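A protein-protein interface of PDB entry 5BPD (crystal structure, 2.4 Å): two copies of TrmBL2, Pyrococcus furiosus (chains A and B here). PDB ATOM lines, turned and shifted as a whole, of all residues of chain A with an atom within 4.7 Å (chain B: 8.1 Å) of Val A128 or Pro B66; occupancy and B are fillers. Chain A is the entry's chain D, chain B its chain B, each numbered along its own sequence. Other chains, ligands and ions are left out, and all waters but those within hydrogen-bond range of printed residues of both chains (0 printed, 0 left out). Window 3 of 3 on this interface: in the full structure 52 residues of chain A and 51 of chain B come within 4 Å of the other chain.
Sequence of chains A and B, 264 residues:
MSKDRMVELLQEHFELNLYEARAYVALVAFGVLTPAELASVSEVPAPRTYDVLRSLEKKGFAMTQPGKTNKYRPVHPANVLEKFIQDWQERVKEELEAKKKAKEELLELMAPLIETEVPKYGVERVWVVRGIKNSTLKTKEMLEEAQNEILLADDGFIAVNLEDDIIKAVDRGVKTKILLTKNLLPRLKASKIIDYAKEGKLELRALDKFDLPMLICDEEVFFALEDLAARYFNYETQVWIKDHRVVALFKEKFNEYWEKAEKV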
ATOM      1  N   VAL A 126       2.051 -17.859  25.488  1.00  0.00           N
ATOM      2  CA  VAL A 126       2.288 -17.659  24.065  1.00  0.00           C
ATOM      3  C   VAL A 126       3.755 -17.913  23.710  1.00  0.00           C
ATOM      4  O   VAL A 126       4.663 -17.470  24.415  1.00  0.00           O
ATOM      5  CB  VAL A 126       1.846 -16.240  23.628  1.00  0.00           C
ATOM      6  CG1 VAL A 126       2.558 -15.182  24.449  1.00  0.00           C
ATOM      7  CG2 VAL A 126       2.095 -16.033  22.139  1.00  0.00           C
ATOM      8  N   TRP A 127       3.973 -18.646  22.621  1.00  0.00           N
ATOM      9  CA  TRP A 127       5.309 -18.887  22.082  1.00  0.00           C
ATOM     10  C   TRP A 127       5.268 -18.885  20.558  1.00  0.00           C
ATOM     11  O   TRP A 127       4.218 -19.118  19.961  1.00  0.00           O
ATOM     12  CB  TRP A 127       5.871 -20.219  22.589  1.00  0.00           C
ATOM     13  CG  TRP A 127       6.226 -20.189  24.037  1.00  0.00           C
ATOM     14  CD1 TRP A 127       5.542 -20.771  25.058  1.00  0.00           C
ATOM     15  CD2 TRP A 127       7.346 -19.521  24.632  1.00  0.00           C
ATOM     16  NE1 TRP A 127       6.169 -20.518  26.254  1.00  0.00           N
ATOM     17  CE2 TRP A 127       7.280 -19.754  26.020  1.00  0.00           C
ATOM     18  CE3 TRP A 127       8.400 -18.756  24.125  1.00  0.00           C
ATOM     19  CZ2 TRP A 127       8.226 -19.246  26.909  1.00  0.00           C
ATOM     20  CZ3 TRP A 127       9.340 -18.254  25.009  1.00  0.00           C
ATOM     21  CH2 TRP A 127       9.247 -18.502  26.384  1.00  0.00           C
ATOM     22  N   VAL A 128       6.405 -18.626  19.927  1.00  0.00           N
ATOM     23  CA  VAL A 128       6.469 -18.648  18.474  1.00  0.00           C
ATOM     24  C   VAL A 128       7.477 -19.681  18.029  1.00  0.00           C
ATOM     25  O   VAL A 128       8.539 -19.809  18.628  1.00  0.00           O
ATOM     26  CB  VAL A 128       6.820 -17.259  17.889  1.00  0.00           C
ATOM     27  CG1 VAL A 128       7.092 -17.377  16.398  1.00  0.00           C
ATOM     28  CG2 VAL A 128       5.694 -16.277  18.151  1.00  0.00           C
ATOM     29  N   VAL A 129       7.141 -20.412  16.970  1.00  0.00           N
ATOM     30  CA  VAL A 129       8.046 -21.395  16.397  1.00  0.00           C
ATOM     31  C   VAL A 129       8.279 -21.092  14.922  1.00  0.00           C
ATOM     32  O   VAL A 129       7.330 -20.891  14.163  1.00  0.00           O
ATOM     33  CB  VAL A 129       7.512 -22.831  16.591  1.00  0.00           C
ATOM     34  CG1 VAL A 129       8.377 -23.823  15.844  1.00  0.00           C
ATOM     35  CG2 VAL A 129       7.464 -23.169  18.065  1.00  0.00           C
ATOM     36  N   ARG A 130       9.550 -21.064  14.527  1.00  0.00           N
ATOM     37  CA  ARG A 130       9.936 -20.762  13.153  1.00  0.00           C
ATOM     38  C   ARG A 130      10.066 -22.027  12.309  1.00  0.00           C
ATOM     39  O   ARG A 130      10.719 -22.984  12.716  1.00  0.00           O
ATOM     40  CB  ARG A 130      11.255 -19.990  13.135  1.00  0.00           C
ATOM     41  CG  ARG A 130      11.276 -18.784  14.049  1.00  0.00           C
ATOM     42  CD  ARG A 130      10.534 -17.604  13.443  1.00  0.00           C
ATOM     43  NE  ARG A 130      10.536 -16.455  14.344  1.00  0.00           N
ATOM     44  CZ  ARG A 130       9.835 -15.345  14.143  1.00  0.00           C
ATOM     45  NH1 ARG A 130       9.074 -15.225  13.064  1.00  0.00           N
ATOM     46  NH2 ARG A 130       9.892 -14.358  15.026  1.00  0.00           N
ATOM     47  N   THR A 237       6.112 -18.287  10.395  1.00  0.00           N
ATOM     48  CA  THR A 237       5.781 -18.054  11.790  1.00  0.00           C
ATOM     49  C   THR A 237       4.563 -18.865  12.204  1.00  0.00           C
ATOM     50  O   THR A 237       3.537 -18.852  11.528  1.00  0.00           O
ATOM     51  CB  THR A 237       5.512 -16.563  12.059  1.00  0.00           C
ATOM     52  OG1 THR A 237       6.683 -15.800  11.737  1.00  0.00           O
ATOM     53  CG2 THR A 237       5.138 -16.337  13.513  1.00  0.00           C
ATOM     54  N   GLN A 238       4.688 -19.569  13.323  1.00  0.00           N
ATOM     55  CA  GLN A 238       3.583 -20.339  13.881  1.00  0.00           C
ATOM     56  C   GLN A 238       3.353 -19.904  15.320  1.00  0.00           C
ATOM     57  O   GLN A 238       4.311 -19.684  16.059  1.00  0.00           O
ATOM     58  CB  GLN A 238       3.878 -21.840  13.793  1.00  0.00           C
ATOM     59  CG  GLN A 238       4.042 -22.343  12.362  1.00  0.00           C
ATOM     60  CD  GLN A 238       4.758 -23.676  12.281  1.00  0.00           C
ATOM     61  OE1 GLN A 238       4.195 -24.671  11.825  1.00  0.00           O
ATOM     62  NE2 GLN A 238       6.016 -23.696  12.706  1.00  0.00           N
ATOM     63  N   GLU B  57      16.557 -20.500  17.338  1.00  0.00           N
ATOM     64  CA  GLU B  57      15.154 -20.353  16.977  1.00  0.00           C
ATOM     65  C   GLU B  57      14.876 -20.953  15.599  1.00  0.00           C
ATOM     66  O   GLU B  57      13.871 -21.634  15.399  1.00  0.00           O
ATOM     67  CB  GLU B  57      14.762 -18.874  17.015  1.00  0.00           C
ATOM     68  CG  GLU B  57      13.350 -18.563  16.554  1.00  0.00           C
ATOM     69  CD  GLU B  57      13.058 -17.072  16.572  1.00  0.00           C
ATOM     70  OE1 GLU B  57      13.710 -16.348  17.353  1.00  0.00           O
ATOM     71  OE2 GLU B  57      12.185 -16.624  15.800  1.00  0.00           O
ATOM     72  N   ALA B  62      14.681 -23.790  19.934  1.00  0.00           N
ATOM     73  CA  ALA B  62      14.087 -22.841  20.867  1.00  0.00           C
ATOM     74  C   ALA B  62      12.774 -22.270  20.347  1.00  0.00           C
ATOM     75  O   ALA B  62      12.522 -22.251  19.144  1.00  0.00           O
ATOM     76  CB  ALA B  62      15.070 -21.712  21.168  1.00  0.00           C
ATOM     77  N   MET B  63      11.931 -21.836  21.277  1.00  0.00           N
ATOM     78  CA  MET B  63      10.741 -21.064  20.948  1.00  0.00           C
ATOM     79  C   MET B  63      10.896 -19.685  21.576  1.00  0.00           C
ATOM     80  O   MET B  63      11.574 -19.535  22.593  1.00  0.00           O
ATOM     81  CB  MET B  63       9.474 -21.755  21.448  1.00  0.00           C
ATOM     82  CG  MET B  63       9.372 -23.216  21.046  1.00  0.00           C
ATOM     83  SD  MET B  63       7.893 -24.024  21.686  1.00  0.00           S
ATOM     84  CE  MET B  63       8.067 -25.658  20.976  1.00  0.00           C
ATOM     85  N   THR B  64      10.281 -18.672  20.979  1.00  0.00           N
ATOM     86  CA  THR B  64      10.536 -17.315  21.436  1.00  0.00           C
ATOM     87  C   THR B  64       9.266 -16.491  21.590  1.00  0.00           C
ATOM     88  O   THR B  64       8.245 -16.754  20.952  1.00  0.00           O
ATOM     89  CB  THR B  64      11.502 -16.577  20.472  1.00  0.00           C
ATOM     90  OG1 THR B  64      11.742 -15.250  20.953  1.00  0.00           O
ATOM     91  CG2 THR B  64      10.921 -16.507  19.070  1.00  0.00           C
ATOM     92  N   GLN B  65       9.341 -15.502  22.471  1.00  0.00           N
ATOM     93  CA  GLN B  65       8.342 -14.451  22.525  1.00  0.00           C
ATOM     94  C   GLN B  65       8.940 -13.175  21.943  1.00  0.00           C
ATOM     95  O   GLN B  65       9.677 -12.466  22.627  1.00  0.00           O
ATOM     96  CB  GLN B  65       7.874 -14.213  23.957  1.00  0.00           C
ATOM     97  CG  GLN B  65       7.091 -15.353  24.560  1.00  0.00           C
ATOM     98  CD  GLN B  65       6.419 -14.947  25.850  1.00  0.00           C
ATOM     99  OE1 GLN B  65       6.562 -13.812  26.300  1.00  0.00           O
ATOM    100  NE2 GLN B  65       5.671 -15.869  26.448  1.00  0.00           N
ATOM    101  N   PRO B  66       8.637 -12.884  20.672  1.00  0.00           N
ATOM    102  CA  PRO B  66       9.154 -11.662  20.044  1.00  0.00           C
ATOM    103  C   PRO B  66       8.655 -10.405  20.742  1.00  0.00           C
ATOM    104  O   PRO B  66       7.454 -10.273  20.978  1.00  0.00           O
ATOM    105  CB  PRO B  66       8.611 -11.741  18.615  1.00  0.00           C
ATOM    106  CG  PRO B  66       8.365 -13.201  18.387  1.00  0.00           C
ATOM    107  CD  PRO B  66       7.908 -13.731  19.714  1.00  0.00           C
ATOM    108  N   GLY B  67       9.573  -9.506  21.083  1.00  0.00           N
ATOM    109  CA  GLY B  67       9.219  -8.254  21.729  1.00  0.00           C
ATOM    110  C   GLY B  67      10.425  -7.389  22.038  1.00  0.00           C
ATOM    111  O   GLY B  67      11.536  -7.679  21.593  1.00  0.00           O
ATOM    112  N   LYS B  68      10.208  -6.308  22.784  1.00  0.00           N
ATOM    113  CA  LYS B  68      11.310  -5.458  23.219  1.00  0.00           C
ATOM    114  C   LYS B  68      12.316  -6.309  23.984  1.00  0.00           C
ATOM    115  O   LYS B  68      13.527  -6.186  23.799  1.00  0.00           O
ATOM    116  CB  LYS B  68      10.808  -4.301  24.085  1.00  0.00           C
ATOM    117  CG  LYS B  68      10.177  -3.160  23.300  1.00  0.00           C
ATOM    118  CD  LYS B  68       8.823  -3.548  22.733  1.00  0.00           C
ATOM    119  CE  LYS B  68       8.165  -2.374  22.024  1.00  0.00           C
ATOM    120  NZ  LYS B  68       6.750  -2.664  21.660  1.00  0.00           N
ATOM    121  N   THR B  69      11.795  -7.179  24.840  1.00  0.00           N
ATOM    122  CA  THR B  69      12.622  -8.147  25.546  1.00  0.00           C
ATOM    123  C   THR B  69      12.251  -9.554  25.096  1.00  0.00           C
ATOM    124  O   THR B  69      11.222 -10.094  25.497  1.00  0.00           O
ATOM    125  CB  THR B  69      12.455  -8.034  27.072  1.00  0.00           C
ATOM    126  OG1 THR B  69      11.100  -8.335  27.433  1.00  0.00           O
ATOM    127  CG2 THR B  69      12.801  -6.628  27.541  1.00  0.00           C
ATOM    128  N   ASN B  70      13.093 -10.138  24.251  1.00  0.00           N
ATOM    129  CA  ASN B  70      12.843 -11.474  23.727  1.00  0.00           C
ATOM    130  C   ASN B  70      13.012 -12.524  24.819  1.00  0.00           C
ATOM    131  O   ASN B  70      14.068 -12.611  25.445  1.00  0.00           O
ATOM    132  CB  ASN B  70      13.788 -11.785  22.561  1.00  0.00           C
ATOM    133  CG  ASN B  70      13.656 -10.796  21.420  1.00  0.00           C
ATOM    134  OD1 ASN B  70      12.957 -11.052  20.439  1.00  0.00           O
ATOM    135  ND2 ASN B  70      14.335  -9.660  21.540  1.00  0.00           N
ATOM    136  N   LYS B  71      11.967 -13.311  25.055  1.00  0.00           N
ATOM    137  CA  LYS B  71      12.078 -14.482  25.922  1.00  0.00           C
ATOM    138  C   LYS B  71      12.231 -15.733  25.073  1.00  0.00           C
ATOM    139  O   LYS B  71      11.514 -15.914  24.085  1.00  0.00           O
ATOM    140  CB  LYS B  71      10.859 -14.618  26.838  1.00  0.00           C
ATOM    141  CG  LYS B  71      10.893 -13.729  28.068  1.00  0.00           C
ATOM    142  CD  LYS B  71       9.708 -14.016  28.975  1.00  0.00           C
ATOM    143  CE  LYS B  71       9.704 -13.102  30.188  1.00  0.00           C
ATOM    144  NZ  LYS B  71       8.555 -13.391  31.086  1.00  0.00           N
ATOM    145  N   TYR B  72      13.167 -16.594  25.456  1.00  0.00           N
ATOM    146  CA  TYR B  72      13.379 -17.850  24.749  1.00  0.00           C
ATOM    147  C   TYR B  72      13.195 -19.039  25.686  1.00  0.00           C
ATOM    148  O   TYR B  72      13.712 -19.044  26.807  1.00  0.00           O
ATOM    149  CB  TYR B  72      14.772 -17.888  24.113  1.00  0.00           C
ATOM    150  CG  TYR B  72      14.970 -16.873  23.008  1.00  0.00           C
ATOM    151  CD1 TYR B  72      14.639 -17.174  21.694  1.00  0.00           C
ATOM    152  CD2 TYR B  72      15.489 -15.615  23.278  1.00  0.00           C
ATOM    153  CE1 TYR B  72      14.818 -16.252  20.684  1.00  0.00           C
ATOM    154  CE2 TYR B  72      15.670 -14.687  22.276  1.00  0.00           C
ATOM    155  CZ  TYR B  72      15.333 -15.008  20.981  1.00  0.00           C
ATOM    156  OH  TYR B  72      15.515 -14.079  19.983  1.00  0.00           O
ATOM    157  N   ARG B  73      12.437 -20.034  25.236  1.00  0.00           N
ATOM    158  CA  ARG B  73      12.334 -21.289  25.967  1.00  0.00           C
ATOM    159  C   ARG B  73      12.862 -22.418  25.092  1.00  0.00           C
ATOM    160  O   ARG B  73      12.755 -22.363  23.867  1.00  0.00           O
ATOM    161  CB  ARG B  73      10.892 -21.569  26.397  1.00  0.00           C
ATOM    162  CG  ARG B  73      10.003 -22.219  25.345  1.00  0.00           C
ATOM    163  CD  ARG B  73       8.842 -22.900  26.053  1.00  0.00           C
ATOM    164  NE  ARG B  73       8.131 -23.883  25.242  1.00  0.00           N
ATOM    165  CZ  ARG B  73       8.440 -25.174  25.190  1.00  0.00           C
ATOM    166  NH1 ARG B  73       9.469 -25.637  25.885  1.00  0.00           N
ATOM    167  NH2 ARG B  73       7.733 -26.000  24.432  1.00  0.00           N
ATOM    168  N   VAL B  75      13.144 -26.131  23.300  1.00  0.00           N
ATOM    169  CA  VAL B  75      12.363 -27.273  22.868  1.00  0.00           C
ATOM    170  C   VAL B  75      12.865 -28.480  23.653  1.00  0.00           C
ATOM    171  O   VAL B  75      14.053 -28.572  23.965  1.00  0.00           O
ATOM    172  CB  VAL B  75      12.474 -27.497  21.352  1.00  0.00           C
ATOM    173  CG1 VAL B  75      11.707 -28.745  20.938  1.00  0.00           C
ATOM    174  CG2 VAL B  75      11.971 -26.277  20.600  1.00  0.00           C
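No position is printed for both chains.
Of the 14 printed residues of chain B, 8 touch a printed residue of chain A.
Hydrophobic or aromatic side chains of chain B within 4 Å of the printed part of chain A: Met B63 and Pro B66.
Hydrophobic or aromatic side chains of chain A within 4 Å of the printed part of chain B: Val A126, Trp A127, Val A128 and Val A129.
Among the printed residues, Asp or Glu carboxylates within 4 Å of a Lys or Arg side-chain nitrogen of the other chain: Arg A130 with Glu B57.
OE2 of Glu B57 lies within salt-bridge range of NH2 of Arg A130 (3.3 Å).
The backbone carbonyl oxygen of Thr B64 is in hydrogen-bond range of the backbone NH of Val A128 (2.8 Å).
The side-chain amide nitrogen of Gln B65 sits at hydrogen-bond distance from the backbone carbonyl oxygen of Val A126, 2.8 Å away.
Val A128 touches just these residues of chain B: Met B63 (3.4 Å), Thr B64 (2.8 Å) and Pro B66 (3.7 Å).
Printed residues of chain B within 4 Å of Arg A130: Glu B57 (2.2 Å) and Pro B66 (3.9 Å).
Printed residues of chain A within 4 Å of Met B63: Trp A127, Val A128 and Val A129.
Of the printed residues of chain A, Thr B64 touches Trp A127 (3.5 Å) and Val A128 (2.8 Å).
Of chain A, only Val A128 (3.7 Å) and Arg A130 (3.9 Å) come within 4 Å of Pro B66.
The nearest printed residue of chain B that does not touch Val A126 is Thr B64 (5.0 Å).
N of Met B63 is in hydrogen-bond range of O of Arg B73 (2.8 Å).
O of Lys B71 lies close to OG1 of Thr B64, 3.2 Å away.
The backbone NH of Gln B65 sits at hydrogen-bond distance from the backbone carbonyl oxygen of Lys B71, at 2.7 Å.
N of Val A129 is in hydrogen-bond range of O of Gln A238, 3.1 Å away.
OG1 of Thr A237 is in hydrogen-bond range of NH1 of Arg A130, 2.8 Å away.
O of Met B63 touches CZ3 of Trp A127, 3.5 Å away.
Thr B64 touches Trp A127.
Gln B65 touches Trp A127 (CG to CE3, 3.7 Å).
CZ3 of Trp A127 touches O of Lys B71, 3.3 Å away.
Trp A127 touches Tyr B72 (CZ3 to C, 3.99 Å).
Trp A127 touches Arg B73.
O of Val A128 touches CA of Met B63, at 3.4 Å.
Pro B66 touches Val A128.
Val A129 touches Met B63.
Pro B66 touches Arg A130.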
